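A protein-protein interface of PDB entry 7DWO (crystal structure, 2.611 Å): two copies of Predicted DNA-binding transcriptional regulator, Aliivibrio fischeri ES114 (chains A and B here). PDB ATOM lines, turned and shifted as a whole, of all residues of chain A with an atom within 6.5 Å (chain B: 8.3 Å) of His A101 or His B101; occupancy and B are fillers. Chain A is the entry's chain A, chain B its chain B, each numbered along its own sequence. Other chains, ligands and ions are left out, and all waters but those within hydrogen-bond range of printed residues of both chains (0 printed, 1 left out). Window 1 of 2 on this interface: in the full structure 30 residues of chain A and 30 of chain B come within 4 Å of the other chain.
NE2 of His B101 sits close to NE2 of His A101 (3.4 Å).
A ring nitrogen (ND1) of His A101 is in hydrogen-bond range of the side-chain sulfur of Met B223.
A ring nitrogen (NE2) of His A101 is in hydrogen-bond range of the side-chain carboxylate (OD2) of Asp B225, 2.4 Å away.
The backbone carbonyl oxygen (O) of Ala B104 sits close to the side-chain sulfur (SD) of Met A226 (3.7 Å).
OG1 of Thr A105 lies within hydrogen-bond range of O of His A101 (2.9 Å).
The side-chain hydroxyl of Thr A105 is in hydrogen-bond range of the backbone carbonyl oxygen of Ser A102 (3.0 Å).
The backbone carbonyl oxygen (O) of His B101 lies within hydrogen-bond range of the side-chain hydroxyl (OG1) of Thr B105, 3.2 Å away.
The backbone carbonyl oxygen (O) of Ser B102 sits at hydrogen-bond distance from the side-chain hydroxyl (OG1) of Thr B105 (3.0 Å).
OG of Ser B221 is in hydrogen-bond range of N of Met B223 (3.1 Å).
SD of Met B226 touches O of Ala A104, at 3.9 Å.
Asp B225 touches Thr A105.
CD1 of Ile B229 touches CB of Thr A105, 3.8 Å away.
SD of Met A223 touches CD2 of His B101, 3.6 Å away.
Met A223 touches Ala B104 (CE to CB, 3.95 Å).
CG1 of Val B126 touches CE of Met A223, at 3.7 Å.
CE1 of His B101 touches OD2 of Asp A225 (3.5 Å).
Thr B105 touches Asp A225.
Met A226 touches Thr B105 (SD to CA, 3.9 Å).
SD of Met A226 touches CD1 of Ile B108, 3.7 Å away.
His A101 touches three residues of chain B.
His B101 touches three residues of chain A.
No residue of chain B comes within 4 Å of Ala A100.
No residue of chain B comes within 4 Å of Ser A102.
Of the printed residues of chain B, Met A226 touches Ala B104 (3.7 Å), Thr B105 (3.9 Å) and Ile B108 (3.7 Å).
Of the printed residues of chain A, Ile B229 touches Thr A105.
Printed residues of chain B within 4 Å of Asp A225: His B101 (3.5 Å) and Thr B105 (3.97 Å).
Of the printed residues of chain B, Met A223 touches His B101, Ala B104 and Val B126.
The nearest printed residue of chain B that does not touch Ala A104 is Met B223 (4.1 Å).
Hydrophobic or aromatic side chains of chain B within 4 Å of the printed part of chain A: His B101, Ala B104, Ile B108, Val B126, Met B223, Met B226 and Ile B229.
Along chain A the printed residues that touch a printed residue of chain B span positions 101 to 226.
Among the printed residues, no Asp or Glu carboxylate lies within 4 Å of a Lys or Arg side-chain nitrogen of the other chain.
His A101 touches its own counterpart, His B101.
His A101 touches Met B223, and with the chains exchanged Met A223 touches His B101.
His A101 touches Asp B225, and with the chains exchanged Asp A225 touches His B101.
Met A226 touches Thr B105, but with the chains exchanged Thr A105 does not touch Met B226 (4.04 Å).
15 positions are printed for both chains.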
ATOM      1  N   ALA A  99     -21.094   8.415 -20.006  1.00  0.00           N
ATOM      2  CA  ALA A  99     -22.234   8.611 -19.124  1.00  0.00           C
ATOM      3  C   ALA A  99     -23.430   9.130 -19.902  1.00  0.00           C
ATOM      4  O   ALA A  99     -23.276   9.892 -20.860  1.00  0.00           O
ATOM      5  CB  ALA A  99     -21.897   9.590 -17.992  1.00  0.00           C
ATOM      6  N   ALA A 100     -24.620   8.697 -19.491  1.00  0.00           N
ATOM      7  CA  ALA A 100     -25.839   9.337 -19.960  1.00  0.00           C
ATOM      8  C   ALA A 100     -25.837  10.794 -19.517  1.00  0.00           C
ATOM      9  O   ALA A 100     -25.406  11.118 -18.407  1.00  0.00           O
ATOM     10  CB  ALA A 100     -27.068   8.609 -19.417  1.00  0.00           C
ATOM     11  N   HIS A 101     -26.310  11.675 -20.400  1.00  0.00           N
ATOM     12  CA  HIS A 101     -26.160  13.112 -20.185  1.00  0.00           C
ATOM     13  C   HIS A 101     -26.745  13.539 -18.842  1.00  0.00           C
ATOM     14  O   HIS A 101     -26.094  14.246 -18.062  1.00  0.00           O
ATOM     15  CB  HIS A 101     -26.817  13.876 -21.334  1.00  0.00           C
ATOM     16  CG  HIS A 101     -26.433  15.320 -21.403  1.00  0.00           C
ATOM     17  ND1 HIS A 101     -25.512  15.801 -22.308  1.00  0.00           N
ATOM     18  CD2 HIS A 101     -26.846  16.389 -20.681  1.00  0.00           C
ATOM     19  CE1 HIS A 101     -25.375  17.105 -22.142  1.00  0.00           C
ATOM     20  NE2 HIS A 101     -26.172  17.486 -21.163  1.00  0.00           N
ATOM     21  N   SER A 102     -27.977  13.109 -18.555  1.00  0.00           N
ATOM     22  CA  SER A 102     -28.616  13.471 -17.293  1.00  0.00           C
ATOM     23  C   SER A 102     -27.844  12.910 -16.109  1.00  0.00           C
ATOM     24  O   SER A 102     -27.584  13.620 -15.128  1.00  0.00           O
ATOM     25  CB  SER A 102     -30.060  12.972 -17.274  1.00  0.00           C
ATOM     26  OG  SER A 102     -30.118  11.574 -17.495  1.00  0.00           O
ATOM     27  N   LEU A 103     -27.475  11.629 -16.179  1.00  0.00           N
ATOM     28  CA  LEU A 103     -26.699  11.024 -15.105  1.00  0.00           C
ATOM     29  C   LEU A 103     -25.373  11.741 -14.918  1.00  0.00           C
ATOM     30  O   LEU A 103     -24.935  11.962 -13.785  1.00  0.00           O
ATOM     31  CB  LEU A 103     -26.466   9.542 -15.392  1.00  0.00           C
ATOM     32  CG  LEU A 103     -27.711   8.663 -15.480  1.00  0.00           C
ATOM     33  CD1 LEU A 103     -27.310   7.213 -15.685  1.00  0.00           C
ATOM     34  CD2 LEU A 103     -28.562   8.824 -14.230  1.00  0.00           C
ATOM     35  N   ALA A 104     -24.718  12.111 -16.019  1.00  0.00           N
ATOM     36  CA  ALA A 104     -23.456  12.834 -15.928  1.00  0.00           C
ATOM     37  C   ALA A 104     -23.638  14.150 -15.182  1.00  0.00           C
ATOM     38  O   ALA A 104     -23.004  14.390 -14.146  1.00  0.00           O
ATOM     39  CB  ALA A 104     -22.890  13.076 -17.329  1.00  0.00           C
ATOM     40  N   THR A 105     -24.533  15.004 -15.689  1.00  0.00           N
ATOM     41  CA  THR A 105     -24.751  16.312 -15.080  1.00  0.00           C
ATOM     42  C   THR A 105     -25.232  16.200 -13.639  1.00  0.00           C
ATOM     43  O   THR A 105     -25.019  17.120 -12.842  1.00  0.00           O
ATOM     44  CB  THR A 105     -25.756  17.114 -15.908  1.00  0.00           C
ATOM     45  OG1 THR A 105     -26.925  16.319 -16.138  1.00  0.00           O
ATOM     46  CG2 THR A 105     -25.153  17.511 -17.244  1.00  0.00           C
ATOM     47  N   SER A 106     -25.875  15.085 -13.280  1.00  0.00           N
ATOM     48  CA  SER A 106     -26.388  14.942 -11.923  1.00  0.00           C
ATOM     49  C   SER A 106     -25.324  14.432 -10.959  1.00  0.00           C
ATOM     50  O   SER A 106     -25.244  14.898  -9.817  1.00  0.00           O
ATOM     51  CB  SER A 106     -27.597  14.005 -11.920  1.00  0.00           C
ATOM     52  OG  SER A 106     -28.066  13.780 -10.603  1.00  0.00           O
ATOM     53  N   ALA A 128     -20.553  11.678 -23.539  1.00  0.00           N
ATOM     54  CA  ALA A 128     -21.890  11.118 -23.668  1.00  0.00           C
ATOM     55  C   ALA A 128     -21.832   9.706 -24.246  1.00  0.00           C
ATOM     56  O   ALA A 128     -20.986   9.387 -25.085  1.00  0.00           O
ATOM     57  CB  ALA A 128     -22.762  12.010 -24.549  1.00  0.00           C
ATOM     58  N   ILE A 129     -22.754   8.860 -23.788  1.00  0.00           N
ATOM     59  CA  ILE A 129     -22.742   7.452 -24.162  1.00  0.00           C
ATOM     60  C   ILE A 129     -23.110   7.296 -25.631  1.00  0.00           C
ATOM     61  O   ILE A 129     -24.075   7.901 -26.116  1.00  0.00           O
ATOM     62  CB  ILE A 129     -23.704   6.650 -23.274  1.00  0.00           C
ATOM     63  CG1 ILE A 129     -23.125   6.462 -21.877  1.00  0.00           C
ATOM     64  CG2 ILE A 129     -24.003   5.293 -23.887  1.00  0.00           C
ATOM     65  CD1 ILE A 129     -24.076   5.770 -20.927  1.00  0.00           C
ATOM     66  N   LEU A 147     -21.534   5.158 -16.818  1.00  0.00           N
ATOM     67  CA  LEU A 147     -22.667   5.606 -16.007  1.00  0.00           C
ATOM     68  C   LEU A 147     -23.915   5.544 -16.875  1.00  0.00           C
ATOM     69  O   LEU A 147     -24.152   6.429 -17.701  1.00  0.00           O
ATOM     70  CB  LEU A 147     -22.434   7.014 -15.475  1.00  0.00           C
ATOM     71  CG  LEU A 147     -21.266   7.177 -14.507  1.00  0.00           C
ATOM     72  CD1 LEU A 147     -21.284   8.564 -13.881  1.00  0.00           C
ATOM     73  CD2 LEU A 147     -21.328   6.094 -13.446  1.00  0.00           C
ATOM     74  N   MET A 223     -32.880  13.931 -25.417  1.00  0.00           N
ATOM     75  CA  MET A 223     -32.202  14.778 -24.443  1.00  0.00           C
ATOM     76  C   MET A 223     -33.214  15.238 -23.403  1.00  0.00           C
ATOM     77  O   MET A 223     -34.056  16.096 -23.686  1.00  0.00           O
ATOM     78  CB  MET A 223     -31.558  15.973 -25.136  1.00  0.00           C
ATOM     79  CG  MET A 223     -30.599  15.611 -26.247  1.00  0.00           C
ATOM     80  SD  MET A 223     -30.072  17.070 -27.159  1.00  0.00           S
ATOM     81  CE  MET A 223     -31.595  17.533 -27.975  1.00  0.00           C
ATOM     82  N   THR A 224     -33.134  14.675 -22.196  1.00  0.00           N
ATOM     83  CA  THR A 224     -34.049  15.095 -21.138  1.00  0.00           C
ATOM     84  C   THR A 224     -33.836  16.556 -20.767  1.00  0.00           C
ATOM     85  O   THR A 224     -34.759  17.212 -20.274  1.00  0.00           O
ATOM     86  CB  THR A 224     -33.885  14.200 -19.910  1.00  0.00           C
ATOM     87  OG1 THR A 224     -34.788  14.626 -18.882  1.00  0.00           O
ATOM     88  CG2 THR A 224     -32.472  14.279 -19.389  1.00  0.00           C
ATOM     89  N   ASP A 225     -32.632  17.082 -21.003  1.00  0.00           N
ATOM     90  CA  ASP A 225     -32.385  18.509 -20.824  1.00  0.00           C
ATOM     91  C   ASP A 225     -33.288  19.332 -21.737  1.00  0.00           C
ATOM     92  O   ASP A 225     -33.887  20.332 -21.314  1.00  0.00           O
ATOM     93  CB  ASP A 225     -30.912  18.805 -21.108  1.00  0.00           C
ATOM     94  CG  ASP A 225     -30.473  20.151 -20.582  1.00  0.00           C
ATOM     95  OD1 ASP A 225     -31.233  20.760 -19.800  1.00  0.00           O
ATOM     96  OD2 ASP A 225     -29.367  20.597 -20.950  1.00  0.00           O
ATOM     97  N   MET A 226     -33.403  18.912 -23.000  1.00  0.00           N
ATOM     98  CA  MET A 226     -34.248  19.613 -23.961  1.00  0.00           C
ATOM     99  C   MET A 226     -35.712  19.576 -23.535  1.00  0.00           C
ATOM    100  O   MET A 226     -36.411  20.599 -23.570  1.00  0.00           O
ATOM    101  CB  MET A 226     -34.069  18.987 -25.345  1.00  0.00           C
ATOM    102  CG  MET A 226     -34.756  19.722 -26.481  1.00  0.00           C
ATOM    103  SD  MET A 226     -33.881  21.216 -26.977  1.00  0.00           S
ATOM    104  CE  MET A 226     -34.772  22.467 -26.051  1.00  0.00           C
ATOM    105  N   ALA B  98     -30.851  16.785 -36.202  1.00  0.00           N
ATOM    106  CA  ALA B  98     -29.676  16.504 -35.394  1.00  0.00           C
ATOM    107  C   ALA B  98     -29.032  17.828 -35.009  1.00  0.00           C
ATOM    108  O   ALA B  98     -29.001  18.768 -35.808  1.00  0.00           O
ATOM    109  CB  ALA B  98     -28.682  15.626 -36.154  1.00  0.00           C
ATOM    110  N   ALA B  99     -28.539  17.912 -33.778  1.00  0.00           N
ATOM    111  CA  ALA B  99     -28.003  19.185 -33.322  1.00  0.00           C
ATOM    112  C   ALA B  99     -26.931  18.974 -32.266  1.00  0.00           C
ATOM    113  O   ALA B  99     -26.938  17.981 -31.534  1.00  0.00           O
ATOM    114  CB  ALA B  99     -29.107  20.089 -32.761  1.00  0.00           C
ATOM    115  N   ALA B 100     -26.001  19.924 -32.207  1.00  0.00           N
ATOM    116  CA  ALA B 100     -25.131  20.033 -31.048  1.00  0.00           C
ATOM    117  C   ALA B 100     -25.974  20.374 -29.827  1.00  0.00           C
ATOM    118  O   ALA B 100     -26.960  21.109 -29.922  1.00  0.00           O
ATOM    119  CB  ALA B 100     -24.059  21.098 -31.279  1.00  0.00           C
ATOM    120  N   HIS B 101     -25.580  19.827 -28.675  1.00  0.00           N
ATOM    121  CA  HIS B 101     -26.416  19.912 -27.482  1.00  0.00           C
ATOM    122  C   HIS B 101     -26.744  21.359 -27.129  1.00  0.00           C
ATOM    123  O   HIS B 101     -27.916  21.723 -26.967  1.00  0.00           O
ATOM    124  CB  HIS B 101     -25.720  19.214 -26.314  1.00  0.00           C
ATOM    125  CG  HIS B 101     -26.662  18.661 -25.294  1.00  0.00           C
ATOM    126  ND1 HIS B 101     -27.260  19.445 -24.331  1.00  0.00           N
ATOM    127  CD2 HIS B 101     -27.114  17.402 -25.089  1.00  0.00           C
ATOM    128  CE1 HIS B 101     -28.037  18.690 -23.575  1.00  0.00           C
ATOM    129  NE2 HIS B 101     -27.967  17.446 -24.014  1.00  0.00           N
ATOM    130  N   SER B 102     -25.716  22.204 -27.014  1.00  0.00           N
ATOM    131  CA  SER B 102     -25.944  23.598 -26.649  1.00  0.00           C
ATOM    132  C   SER B 102     -26.743  24.327 -27.720  1.00  0.00           C
ATOM    133  O   SER B 102     -27.636  25.124 -27.404  1.00  0.00           O
ATOM    134  CB  SER B 102     -24.608  24.301 -26.399  1.00  0.00           C
ATOM    135  OG  SER B 102     -23.710  24.106 -27.477  1.00  0.00           O
ATOM    136  N   LEU B 103     -26.442  24.064 -28.995  1.00  0.00           N
ATOM    137  CA  LEU B 103     -27.213  24.672 -30.076  1.00  0.00           C
ATOM    138  C   LEU B 103     -28.679  24.276 -29.992  1.00  0.00           C
ATOM    139  O   LEU B 103     -29.568  25.120 -30.161  1.00  0.00           O
ATOM    140  CB  LEU B 103     -26.635  24.272 -31.432  1.00  0.00           C
ATOM    141  CG  LEU B 103     -25.250  24.815 -31.775  1.00  0.00           C
ATOM    142  CD1 LEU B 103     -24.906  24.478 -33.213  1.00  0.00           C
ATOM    143  CD2 LEU B 103     -25.193  26.317 -31.538  1.00  0.00           C
ATOM    144  N   ALA B 104     -28.951  22.996 -29.737  1.00  0.00           N
ATOM    145  CA  ALA B 104     -30.327  22.541 -29.572  1.00  0.00           C
ATOM    146  C   ALA B 104     -31.015  23.288 -28.437  1.00  0.00           C
ATOM    147  O   ALA B 104     -32.036  23.960 -28.640  1.00  0.00           O
ATOM    148  CB  ALA B 104     -30.345  21.031 -29.323  1.00  0.00           C
ATOM    149  N   THR B 105     -30.445  23.201 -27.230  1.00  0.00           N
ATOM    150  CA  THR B 105     -31.062  23.816 -26.059  1.00  0.00           C
ATOM    151  C   THR B 105     -31.215  25.326 -26.198  1.00  0.00           C
ATOM    152  O   THR B 105     -32.085  25.911 -25.544  1.00  0.00           O
ATOM    153  CB  THR B 105     -30.248  23.496 -24.801  1.00  0.00           C
ATOM    154  OG1 THR B 105     -28.923  24.024 -24.938  1.00  0.00           O
ATOM    155  CG2 THR B 105     -30.172  21.992 -24.581  1.00  0.00           C
ATOM    156  N   SER B 106     -30.402  25.971 -27.036  1.00  0.00           N
ATOM    157  CA  SER B 106     -30.499  27.414 -27.203  1.00  0.00           C
ATOM    158  C   SER B 106     -31.485  27.824 -28.292  1.00  0.00           C
ATOM    159  O   SER B 106     -32.221  28.802 -28.121  1.00  0.00           O
ATOM    160  CB  SER B 106     -29.120  27.998 -27.514  1.00  0.00           C
ATOM    161  OG  SER B 106     -29.192  29.402 -27.691  1.00  0.00           O
ATOM    162  N   LEU B 107     -31.523  27.099 -29.410  1.00  0.00           N
ATOM    163  CA  LEU B 107     -32.290  27.537 -30.569  1.00  0.00           C
ATOM    164  C   LEU B 107     -33.696  26.952 -30.615  1.00  0.00           C
ATOM    165  O   LEU B 107     -34.628  27.633 -31.053  1.00  0.00           O
ATOM    166  CB  LEU B 107     -31.546  27.173 -31.857  1.00  0.00           C
ATOM    167  CG  LEU B 107     -30.178  27.819 -32.076  1.00  0.00           C
ATOM    168  CD1 LEU B 107     -29.539  27.296 -33.352  1.00  0.00           C
ATOM    169  CD2 LEU B 107     -30.305  29.334 -32.120  1.00  0.00           C
ATOM    170  N   ILE B 108     -33.875  25.708 -30.180  1.00  0.00           N
ATOM    171  CA  ILE B 108     -35.138  25.001 -30.378  1.00  0.00           C
ATOM    172  C   ILE B 108     -36.313  25.634 -29.632  1.00  0.00           C
ATOM    173  O   ILE B 108     -37.435  25.589 -30.149  1.00  0.00           O
ATOM    174  CB  ILE B 108     -34.970  23.521 -30.009  1.00  0.00           C
ATOM    175  CG1 ILE B 108     -34.026  22.875 -31.013  1.00  0.00           C
ATOM    176  CG2 ILE B 108     -36.302  22.788 -30.002  1.00  0.00           C
ATOM    177  CD1 ILE B 108     -33.602  21.535 -30.609  1.00  0.00           C
ATOM    178  N   VAL B 126     -35.728  15.972 -32.245  1.00  0.00           N
ATOM    179  CA  VAL B 126     -34.364  16.473 -32.123  1.00  0.00           C
ATOM    180  C   VAL B 126     -33.505  15.437 -31.418  1.00  0.00           C
ATOM    181  O   VAL B 126     -33.884  14.916 -30.363  1.00  0.00           O
ATOM    182  CB  VAL B 126     -34.318  17.809 -31.367  1.00  0.00           C
ATOM    183  CG1 VAL B 126     -32.887  18.322 -31.341  1.00  0.00           C
ATOM    184  CG2 VAL B 126     -35.263  18.808 -32.015  1.00  0.00           C
ATOM    185  N   GLU B 127     -32.337  15.163 -31.991  1.00  0.00           N
ATOM    186  CA  GLU B 127     -31.386  14.228 -31.414  1.00  0.00           C
ATOM    187  C   GLU B 127     -29.997  14.852 -31.389  1.00  0.00           C
ATOM    188  O   GLU B 127     -29.649  15.672 -32.247  1.00  0.00           O
ATOM    189  CB  GLU B 127     -31.354  12.903 -32.191  1.00  0.00           C
ATOM    190  CG  GLU B 127     -32.694  12.183 -32.249  1.00  0.00           C
ATOM    191  CD  GLU B 127     -33.179  11.728 -30.884  1.00  0.00           C
ATOM    192  OE1 GLU B 127     -32.341  11.574 -29.970  1.00  0.00           O
ATOM    193  OE2 GLU B 127     -34.401  11.520 -30.724  1.00  0.00           O
ATOM    194  N   ALA B 128     -29.213  14.454 -30.389  1.00  0.00           N
ATOM    195  CA  ALA B 128     -27.841  14.927 -30.277  1.00  0.00           C
ATOM    196  C   ALA B 128     -27.043  14.526 -31.510  1.00  0.00           C
ATOM    197  O   ALA B 128     -27.181  13.414 -32.027  1.00  0.00           O
ATOM    198  CB  ALA B 128     -27.186  14.365 -29.014  1.00  0.00           C
ATOM    199  N   ILE B 129     -26.204  15.448 -31.982  1.00  0.00           N
ATOM    200  CA  ILE B 129     -25.460  15.232 -33.215  1.00  0.00           C
ATOM    201  C   ILE B 129     -24.470  14.089 -33.032  1.00  0.00           C
ATOM    202  O   ILE B 129     -23.794  13.981 -32.002  1.00  0.00           O
ATOM    203  CB  ILE B 129     -24.751  16.530 -33.641  1.00  0.00           C
ATOM    204  CG1 ILE B 129     -23.995  16.329 -34.954  1.00  0.00           C
ATOM    205  CG2 ILE B 129     -23.802  17.017 -32.552  1.00  0.00           C
ATOM    206  CD1 ILE B 129     -23.212  17.545 -35.398  1.00  0.00           C
ATOM    207  N   LEU B 147     -28.248  21.210 -37.014  1.00  0.00           N
ATOM    208  CA  LEU B 147     -27.762  22.422 -36.361  1.00  0.00           C
ATOM    209  C   LEU B 147     -26.360  22.145 -35.838  1.00  0.00           C
ATOM    210  O   LEU B 147     -26.191  21.381 -34.881  1.00  0.00           O
ATOM    211  CB  LEU B 147     -28.696  22.845 -35.232  1.00  0.00           C
ATOM    212  CG  LEU B 147     -30.139  23.155 -35.626  1.00  0.00           C
ATOM    213  CD1 LEU B 147     -30.865  23.863 -34.490  1.00  0.00           C
ATOM    214  CD2 LEU B 147     -30.171  23.987 -36.896  1.00  0.00           C
ATOM    215  N   ALA B 148     -25.349  22.756 -36.455  1.00  0.00           N
ATOM    216  CA  ALA B 148     -23.984  22.401 -36.091  1.00  0.00           C
ATOM    217  C   ALA B 148     -23.064  23.597 -36.272  1.00  0.00           C
ATOM    218  O   ALA B 148     -23.394  24.559 -36.966  1.00  0.00           O
ATOM    219  CB  ALA B 148     -23.472  21.212 -36.913  1.00  0.00           C
ATOM    220  N   PHE B 149     -21.888  23.508 -35.658  1.00  0.00           N
ATOM    221  CA  PHE B 149     -20.899  24.569 -35.767  1.00  0.00           C
ATOM    222  C   PHE B 149     -20.283  24.576 -37.164  1.00  0.00           C
ATOM    223  O   PHE B 149     -20.642  23.788 -38.043  1.00  0.00           O
ATOM    224  CB  PHE B 149     -19.831  24.405 -34.691  1.00  0.00           C
ATOM    225  CG  PHE B 149     -20.346  24.606 -33.296  1.00  0.00           C
ATOM    226  CD1 PHE B 149     -20.593  25.881 -32.816  1.00  0.00           C
ATOM    227  CD2 PHE B 149     -20.585  23.523 -32.467  1.00  0.00           C
ATOM    228  CE1 PHE B 149     -21.070  26.073 -31.534  1.00  0.00           C
ATOM    229  CE2 PHE B 149     -21.064  23.710 -31.183  1.00  0.00           C
ATOM    230  CZ  PHE B 149     -21.306  24.987 -30.717  1.00  0.00           C
ATOM    231  N   SER B 221     -14.309  17.187 -20.971  1.00  0.00           N
ATOM    232  CA  SER B 221     -15.620  16.776 -21.453  1.00  0.00           C
ATOM    233  C   SER B 221     -15.999  17.639 -22.643  1.00  0.00           C
ATOM    234  O   SER B 221     -15.751  18.844 -22.640  1.00  0.00           O
ATOM    235  CB  SER B 221     -16.686  16.894 -20.355  1.00  0.00           C
ATOM    236  OG  SER B 221     -17.967  16.549 -20.852  1.00  0.00           O
ATOM    237  N   SER B 222     -16.594  17.015 -23.657  1.00  0.00           N
ATOM    238  CA  SER B 222     -17.128  17.758 -24.790  1.00  0.00           C
ATOM    239  C   SER B 222     -18.506  18.336 -24.505  1.00  0.00           C
ATOM    240  O   SER B 222     -18.988  19.168 -25.282  1.00  0.00           O
ATOM    241  CB  SER B 222     -17.193  16.862 -26.027  1.00  0.00           C
ATOM    242  OG  SER B 222     -18.050  15.759 -25.803  1.00  0.00           O
ATOM    243  N   MET B 223     -19.148  17.914 -23.418  1.00  0.00           N
ATOM    244  CA  MET B 223     -20.441  18.455 -23.016  1.00  0.00           C
ATOM    245  C   MET B 223     -20.215  19.815 -22.374  1.00  0.00           C
ATOM    246  O   MET B 223     -19.715  19.902 -21.248  1.00  0.00           O
ATOM    247  CB  MET B 223     -21.140  17.503 -22.051  1.00  0.00           C
ATOM    248  CG  MET B 223     -21.429  16.135 -22.628  1.00  0.00           C
ATOM    249  SD  MET B 223     -22.089  15.020 -21.379  1.00  0.00           S
ATOM    250  CE  MET B 223     -20.664  14.818 -20.317  1.00  0.00           C
ATOM    251  N   THR B 224     -20.586  20.882 -23.086  1.00  0.00           N
ATOM    252  CA  THR B 224     -20.296  22.222 -22.590  1.00  0.00           C
ATOM    253  C   THR B 224     -21.129  22.565 -21.359  1.00  0.00           C
ATOM    254  O   THR B 224     -20.694  23.370 -20.528  1.00  0.00           O
ATOM    255  CB  THR B 224     -20.512  23.254 -23.699  1.00  0.00           C
ATOM    256  OG1 THR B 224     -20.117  24.551 -23.232  1.00  0.00           O
ATOM    257  CG2 THR B 224     -21.970  23.292 -24.129  1.00  0.00           C
ATOM    258  N   ASP B 225     -22.311  21.962 -21.210  1.00  0.00           N
ATOM    259  CA  ASP B 225     -23.094  22.199 -20.000  1.00  0.00           C
ATOM    260  C   ASP B 225     -22.454  21.539 -18.785  1.00  0.00           C
ATOM    261  O   ASP B 225     -22.583  22.047 -17.667  1.00  0.00           O
ATOM    262  CB  ASP B 225     -24.531  21.710 -20.189  1.00  0.00           C
ATOM    263  CG  ASP B 225     -24.605  20.254 -20.598  1.00  0.00           C
ATOM    264  OD1 ASP B 225     -23.781  19.824 -21.433  1.00  0.00           O
ATOM    265  OD2 ASP B 225     -25.491  19.539 -20.083  1.00  0.00           O
ATOM    266  N   MET B 226     -21.746  20.426 -18.988  1.00  0.00           N
ATOM    267  CA  MET B 226     -20.976  19.823 -17.904  1.00  0.00           C
ATOM    268  C   MET B 226     -19.892  20.777 -17.414  1.00  0.00           C
ATOM    269  O   MET B 226     -19.738  21.005 -16.204  1.00  0.00           O
ATOM    270  CB  MET B 226     -20.365  18.505 -18.382  1.00  0.00           C
ATOM    271  CG  MET B 226     -19.714  17.663 -17.299  1.00  0.00           C
ATOM    272  SD  MET B 226     -20.912  16.897 -16.190  1.00  0.00           S
ATOM    273  CE  MET B 226     -20.876  18.035 -14.807  1.00  0.00           C
ATOM    274  N   ILE B 229     -21.501  23.633 -15.499  1.00  0.00           N
ATOM    275  CA  ILE B 229     -21.828  23.236 -14.133  1.00  0.00           C
ATOM    276  C   ILE B 229     -20.578  23.252 -13.263  1.00  0.00           C
ATOM    277  O   ILE B 229     -20.585  23.774 -12.141  1.00  0.00           O
ATOM    278  CB  ILE B 229     -22.504  21.853 -14.122  1.00  0.00           C
ATOM    279  CG1 ILE B 229     -23.911  21.938 -14.720  1.00  0.00           C
ATOM    280  CG2 ILE B 229     -22.552  21.289 -12.708  1.00  0.00           C
ATOM    281  CD1 ILE B 229     -24.571  20.591 -14.914  1.00  0.00           C
ATOM    282  N   TYR B 243     -23.898  32.277 -25.853  1.00  0.00           N
ATOM    283  CA  TYR B 243     -25.343  32.088 -25.808  1.00  0.00           C
ATOM    284  C   TYR B 243     -25.796  31.200 -24.656  1.00  0.00           C
ATOM    285  O   TYR B 243     -26.998  31.154 -24.373  1.00  0.00           O
ATOM    286  CB  TYR B 243     -25.841  31.507 -27.135  1.00  0.00           C
ATOM    287  CG  TYR B 243     -25.147  30.232 -27.563  1.00  0.00           C
ATOM    288  CD1 TYR B 243     -25.461  29.012 -26.975  1.00  0.00           C
ATOM    289  CD2 TYR B 243     -24.189  30.246 -28.568  1.00  0.00           C
ATOM    290  CE1 TYR B 243     -24.831  27.848 -27.365  1.00  0.00           C
ATOM    291  CE2 TYR B 243     -23.557  29.085 -28.967  1.00  0.00           C
ATOM    292  CZ  TYR B 243     -23.882  27.888 -28.363  1.00  0.00           C
ATOM    293  OH  TYR B 243     -23.255  26.728 -28.754  1.00  0.00           O
ATOM    294  N   SER B 244     -24.879  30.501 -23.990  1.00  0.00           N
ATOM    295  CA  SER B 244     -25.230  29.538 -22.955  1.00  0.00           C
ATOM    296  C   SER B 244     -24.989  30.055 -21.543  1.00  0.00           C
ATOM    297  O   SER B 244     -25.299  29.344 -20.581  1.00  0.00           O
ATOM    298  CB  SER B 244     -24.445  28.240 -23.164  1.00  0.00           C
ATOM    299  OG  SER B 244     -23.049  28.473 -23.073  1.00  0.00           O
